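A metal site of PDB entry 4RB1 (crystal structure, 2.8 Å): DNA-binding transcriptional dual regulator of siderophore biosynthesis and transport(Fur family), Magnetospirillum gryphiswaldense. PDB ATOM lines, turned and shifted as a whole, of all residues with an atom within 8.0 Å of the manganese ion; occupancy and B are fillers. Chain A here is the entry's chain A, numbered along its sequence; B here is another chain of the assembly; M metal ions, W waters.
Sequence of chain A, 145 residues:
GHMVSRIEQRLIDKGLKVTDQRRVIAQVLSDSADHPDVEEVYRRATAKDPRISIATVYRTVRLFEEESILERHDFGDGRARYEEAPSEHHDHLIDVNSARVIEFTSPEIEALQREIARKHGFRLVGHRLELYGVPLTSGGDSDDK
N of Asp 91 is in hydrogen-bond range of O of Phe 104.
The side-chain amide oxygen (OE1) of Gln 113 sits close to the side-chain carboxylate (OE1) of Glu 110, 3.3 Å away.
The backbone carbonyl oxygen (O) of His 89 sits at hydrogen-bond distance from the side-chain hydroxyl (OG1) of Thr 105.
Along chain A the residues within 4 Å of the manganese ion span positions 89 to 127.
The nearest printed residue that does not touch the manganese ion is Gln 113 (4.4 Å).
The manganese ion is bound by NE2 of His 127 (2.0 Å), water W1 (2.1 Å), OD1 of Asp 91 (2.3 Å), NE2 of His 89 (2.3 Å), OD2 of Asp 91 (2.6 Å) and OE2 of Glu 110 (2.6 Å).
Water W1 bridges the side-chain amide nitrogen (NE2) of Gln 113 and the side-chain carboxylate (OE1) of Glu 110.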
ATOM      1  N   HIS A  89      26.737 -28.134  24.541  1.00  0.00           N
ATOM      2  CA  HIS A  89      25.895 -27.777  23.404  1.00  0.00           C
ATOM      3  C   HIS A  89      26.677 -27.879  22.111  1.00  0.00           C
ATOM      4  O   HIS A  89      27.890 -27.622  22.089  1.00  0.00           O
ATOM      5  CB  HIS A  89      25.323 -26.375  23.589  1.00  0.00           C
ATOM      6  CG  HIS A  89      24.629 -25.835  22.364  1.00  0.00           C
ATOM      7  ND1 HIS A  89      23.342 -26.080  22.090  1.00  0.00           N
ATOM      8  CD2 HIS A  89      25.120 -25.065  21.313  1.00  0.00           C
ATOM      9  CE1 HIS A  89      23.012 -25.489  20.928  1.00  0.00           C
ATOM     10  NE2 HIS A  89      24.104 -24.862  20.463  1.00  0.00           N
ATOM     11  N   HIS A  90      26.016 -28.286  21.035  1.00  0.00           N
ATOM     12  CA  HIS A  90      26.593 -28.215  19.691  1.00  0.00           C
ATOM     13  C   HIS A  90      25.557 -27.926  18.651  1.00  0.00           C
ATOM     14  O   HIS A  90      24.381 -28.348  18.764  1.00  0.00           O
ATOM     15  CB  HIS A  90      27.393 -29.469  19.341  1.00  0.00           C
ATOM     16  CG  HIS A  90      26.544 -30.679  19.114  1.00  0.00           C
ATOM     17  ND1 HIS A  90      26.260 -31.554  20.084  1.00  0.00           N
ATOM     18  CD2 HIS A  90      25.878 -31.132  17.975  1.00  0.00           C
ATOM     19  CE1 HIS A  90      25.471 -32.525  19.598  1.00  0.00           C
ATOM     20  NE2 HIS A  90      25.232 -32.269  18.304  1.00  0.00           N
ATOM     21  N   ASP A  91      25.970 -27.186  17.629  1.00  0.00           N
ATOM     22  CA  ASP A  91      25.141 -26.877  16.484  1.00  0.00           C
ATOM     23  C   ASP A  91      25.542 -27.793  15.348  1.00  0.00           C
ATOM     24  O   ASP A  91      26.421 -28.646  15.504  1.00  0.00           O
ATOM     25  CB  ASP A  91      25.327 -25.419  16.099  1.00  0.00           C
ATOM     26  CG  ASP A  91      25.057 -24.496  17.253  1.00  0.00           C
ATOM     27  OD1 ASP A  91      23.871 -24.418  17.669  1.00  0.00           O
ATOM     28  OD2 ASP A  91      26.023 -23.860  17.768  1.00  0.00           O
ATOM     29  N   HIS A  92      24.892 -27.628  14.195  1.00  0.00           N
ATOM     30  CA  HIS A  92      25.097 -28.558  13.106  1.00  0.00           C
ATOM     31  C   HIS A  92      25.437 -27.927  11.782  1.00  0.00           C
ATOM     32  O   HIS A  92      24.970 -26.829  11.448  1.00  0.00           O
ATOM     33  CB  HIS A  92      23.893 -29.480  12.966  1.00  0.00           C
ATOM     34  CG  HIS A  92      23.634 -30.312  14.196  1.00  0.00           C
ATOM     35  ND1 HIS A  92      22.966 -29.843  15.270  1.00  0.00           N
ATOM     36  CD2 HIS A  92      23.991 -31.629  14.497  1.00  0.00           C
ATOM     37  CE1 HIS A  92      22.899 -30.808  16.201  1.00  0.00           C
ATOM     38  NE2 HIS A  92      23.521 -31.902  15.723  1.00  0.00           N
ATOM     39  N   PHE A 104      29.300 -29.024  15.666  1.00  0.00           N
ATOM     40  CA  PHE A 104      30.317 -28.026  15.909  1.00  0.00           C
ATOM     41  C   PHE A 104      29.911 -27.126  17.057  1.00  0.00           C
ATOM     42  O   PHE A 104      28.729 -26.879  17.285  1.00  0.00           O
ATOM     43  CB  PHE A 104      30.623 -27.204  14.652  1.00  0.00           C
ATOM     44  CG  PHE A 104      29.695 -26.050  14.444  1.00  0.00           C
ATOM     45  CD1 PHE A 104      29.904 -24.841  15.108  1.00  0.00           C
ATOM     46  CD2 PHE A 104      28.607 -26.158  13.577  1.00  0.00           C
ATOM     47  CE1 PHE A 104      29.044 -23.767  14.927  1.00  0.00           C
ATOM     48  CE2 PHE A 104      27.750 -25.085  13.379  1.00  0.00           C
ATOM     49  CZ  PHE A 104      27.970 -23.886  14.051  1.00  0.00           C
ATOM     50  N   THR A 105      30.920 -26.642  17.770  1.00  0.00           N
ATOM     51  CA  THR A 105      30.722 -25.721  18.884  1.00  0.00           C
ATOM     52  C   THR A 105      31.450 -24.399  18.632  1.00  0.00           C
ATOM     53  O   THR A 105      32.575 -24.380  18.129  1.00  0.00           O
ATOM     54  CB  THR A 105      31.151 -26.381  20.225  1.00  0.00           C
ATOM     55  OG1 THR A 105      30.413 -25.786  21.298  1.00  0.00           O
ATOM     56  CG2 THR A 105      32.668 -26.257  20.475  1.00  0.00           C
ATOM     57  N   SER A 106      30.778 -23.300  18.953  1.00  0.00           N
ATOM     58  CA  SER A 106      31.353 -21.963  18.826  1.00  0.00           C
ATOM     59  C   SER A 106      30.962 -21.112  20.038  1.00  0.00           C
ATOM     60  O   SER A 106      29.814 -20.657  20.144  1.00  0.00           O
ATOM     61  CB  SER A 106      30.887 -21.296  17.531  1.00  0.00           C
ATOM     62  OG  SER A 106      31.207 -19.919  17.514  1.00  0.00           O
ATOM     63  N   ILE A 109      29.759 -17.226  19.419  1.00  0.00           N
ATOM     64  CA  ILE A 109      28.440 -17.068  18.804  1.00  0.00           C
ATOM     65  C   ILE A 109      27.322 -17.005  19.856  1.00  0.00           C
ATOM     66  O   ILE A 109      26.500 -16.092  19.807  1.00  0.00           O
ATOM     67  CB  ILE A 109      28.147 -18.161  17.738  1.00  0.00           C
ATOM     68  CG1 ILE A 109      28.809 -17.798  16.408  1.00  0.00           C
ATOM     69  CG2 ILE A 109      26.645 -18.329  17.522  1.00  0.00           C
ATOM     70  CD1 ILE A 109      28.543 -18.776  15.283  1.00  0.00           C
ATOM     71  N   GLU A 110      27.331 -17.951  20.794  1.00  0.00           N
ATOM     72  CA  GLU A 110      26.330 -18.012  21.872  1.00  0.00           C
ATOM     73  C   GLU A 110      26.283 -16.708  22.668  1.00  0.00           C
ATOM     74  O   GLU A 110      25.208 -16.244  23.063  1.00  0.00           O
ATOM     75  CB  GLU A 110      26.639 -19.155  22.838  1.00  0.00           C
ATOM     76  CG  GLU A 110      27.079 -20.448  22.184  1.00  0.00           C
ATOM     77  CD  GLU A 110      26.002 -21.082  21.325  1.00  0.00           C
ATOM     78  OE1 GLU A 110      24.821 -20.703  21.453  1.00  0.00           O
ATOM     79  OE2 GLU A 110      26.357 -21.977  20.526  1.00  0.00           O
ATOM     80  N   GLN A 113      24.751 -14.149  20.583  1.00  0.00           N
ATOM     81  CA  GLN A 113      23.339 -14.507  20.620  1.00  0.00           C
ATOM     82  C   GLN A 113      22.610 -14.025  21.876  1.00  0.00           C
ATOM     83  O   GLN A 113      21.482 -13.529  21.802  1.00  0.00           O
ATOM     84  CB  GLN A 113      23.179 -16.009  20.437  1.00  0.00           C
ATOM     85  CG  GLN A 113      23.635 -16.497  19.067  1.00  0.00           C
ATOM     86  CD  GLN A 113      23.381 -17.968  18.830  1.00  0.00           C
ATOM     87  OE1 GLN A 113      22.889 -18.681  19.714  1.00  0.00           O
ATOM     88  NE2 GLN A 113      23.703 -18.443  17.642  1.00  0.00           N
ATOM     89  N   HIS A 127      17.739 -21.538  21.270  1.00  0.00           N
ATOM     90  CA  HIS A 127      18.112 -21.076  19.941  1.00  0.00           C
ATOM     91  C   HIS A 127      18.283 -22.280  19.058  1.00  0.00           C
ATOM     92  O   HIS A 127      18.245 -23.425  19.533  1.00  0.00           O
ATOM     93  CB  HIS A 127      19.426 -20.326  20.021  1.00  0.00           C
ATOM     94  CG  HIS A 127      20.611 -21.231  20.212  1.00  0.00           C
ATOM     95  ND1 HIS A 127      20.933 -21.771  21.387  1.00  0.00           N
ATOM     96  CD2 HIS A 127      21.531 -21.728  19.285  1.00  0.00           C
ATOM     97  CE1 HIS A 127      22.015 -22.551  21.248  1.00  0.00           C
ATOM     98  NE2 HIS A 127      22.382 -22.520  19.962  1.00  0.00           N
ATOM     99  N   ARG A 128      18.496 -22.031  17.770  1.00  0.00           N
ATOM    100  CA  ARG A 128      18.741 -23.093  16.800  1.00  0.00           C
ATOM    101  C   ARG A 128      19.608 -22.536  15.668  1.00  0.00           C
ATOM    102  O   ARG A 128      19.263 -21.524  15.066  1.00  0.00           O
ATOM    103  CB  ARG A 128      17.415 -23.624  16.279  1.00  0.00           C
ATOM    104  CG  ARG A 128      17.486 -24.355  14.946  1.00  0.00           C
ATOM    105  CD  ARG A 128      16.096 -24.781  14.485  1.00  0.00           C
ATOM    106  NE  ARG A 128      15.872 -24.441  13.084  1.00  0.00           N
ATOM    107  CZ  ARG A 128      15.143 -25.162  12.234  1.00  0.00           C
ATOM    108  NH1 ARG A 128      14.571 -26.305  12.623  1.00  0.00           N
ATOM    109  NH2 ARG A 128      14.992 -24.744  10.989  1.00  0.00           N
ATOM    110  N   LEU A 129      20.735 -23.193  15.420  1.00  0.00           N
ATOM    111  CA  LEU A 129      21.633 -22.800  14.343  1.00  0.00           C
ATOM    112  C   LEU A 129      22.044 -24.014  13.539  1.00  0.00           C
ATOM    113  O   LEU A 129      22.629 -24.954  14.069  1.00  0.00           O
ATOM    114  CB  LEU A 129      22.875 -22.085  14.881  1.00  0.00           C
ATOM    115  CG  LEU A 129      23.972 -21.702  13.863  1.00  0.00           C
ATOM    116  CD1 LEU A 129      23.566 -20.539  12.968  1.00  0.00           C
ATOM    117  CD2 LEU A 129      25.309 -21.392  14.525  1.00  0.00           C
ATOM    118  N   GLU A 130      21.713 -23.997  12.245  1.00  0.00           N
ATOM    119  CA  GLU A 130      22.158 -25.040  11.322  1.00  0.00           C
ATOM    120  C   GLU A 130      22.672 -24.398  10.058  1.00  0.00           C
ATOM    121  O   GLU A 130      22.107 -23.415   9.576  1.00  0.00           O
ATOM    122  CB  GLU A 130      21.063 -26.069  11.036  1.00  0.00           C
ATOM    123  CG  GLU A 130      19.686 -25.466  10.924  1.00  0.00           C
ATOM    124  CD  GLU A 130      18.613 -26.277  11.637  1.00  0.00           C
ATOM    125  OE1 GLU A 130      17.568 -26.549  10.985  1.00  0.00           O
ATOM    126  OE2 GLU A 130      18.815 -26.639  12.823  1.00  0.00           O
ATOM    127  N   LEU B 129      19.327 -19.728  11.308  1.00  0.00           N
ATOM    128  CA  LEU B 129      19.584 -19.305  12.674  1.00  0.00           C
ATOM    129  C   LEU B 129      18.382 -18.584  13.269  1.00  0.00           C
ATOM    130  O   LEU B 129      18.017 -17.487  12.824  1.00  0.00           O
ATOM    131  CB  LEU B 129      20.822 -18.389  12.785  1.00  0.00           C
ATOM    132  CG  LEU B 129      20.877 -17.688  14.155  1.00  0.00           C
ATOM    133  CD1 LEU B 129      21.331 -18.642  15.249  1.00  0.00           C
ATOM    134  CD2 LEU B 129      21.679 -16.395  14.176  1.00  0.00           C
ATOM    135  N   GLU B 130      17.791 -19.189  14.288  1.00  0.00           N
ATOM    136  CA  GLU B 130      16.656 -18.622  14.985  1.00  0.00           C
ATOM    137  C   GLU B 130      16.923 -18.549  16.475  1.00  0.00           C
ATOM    138  O   GLU B 130      17.488 -19.468  17.060  1.00  0.00           O
ATOM    139  CB  GLU B 130      15.409 -19.449  14.745  1.00  0.00           C
ATOM    140  CG  GLU B 130      15.029 -19.616  13.287  1.00  0.00           C
ATOM    141  CD  GLU B 130      14.212 -20.863  13.043  1.00  0.00           C
ATOM    142  OE1 GLU B 130      13.719 -21.042  11.900  1.00  0.00           O
ATOM    143  OE2 GLU B 130      14.063 -21.656  14.010  1.00  0.00           O
ATOM    144  N   LEU B 131      16.506 -17.435  17.054  1.00  0.00           N
ATOM    145  CA  LEU B 131      16.564 -17.221  18.481  1.00  0.00           C
ATOM    146  C   LEU B 131      15.165 -17.231  19.081  1.00  0.00           C
ATOM    147  O   LEU B 131      14.248 -16.628  18.517  1.00  0.00           O
ATOM    148  CB  LEU B 131      17.240 -15.884  18.748  1.00  0.00           C
ATOM    149  CG  LEU B 131      18.768 -15.879  18.894  1.00  0.00           C
ATOM    150  CD1 LEU B 131      19.476 -16.797  17.913  1.00  0.00           C
ATOM    151  CD2 LEU B 131      19.265 -14.448  18.772  1.00  0.00           C
HETATM  152 MN    MN M   1      24.211 -22.884  19.299  1.00  0.00          MN
HETATM  153  O   HOH W   1      24.805 -21.190  18.166  1.00  0.00           O
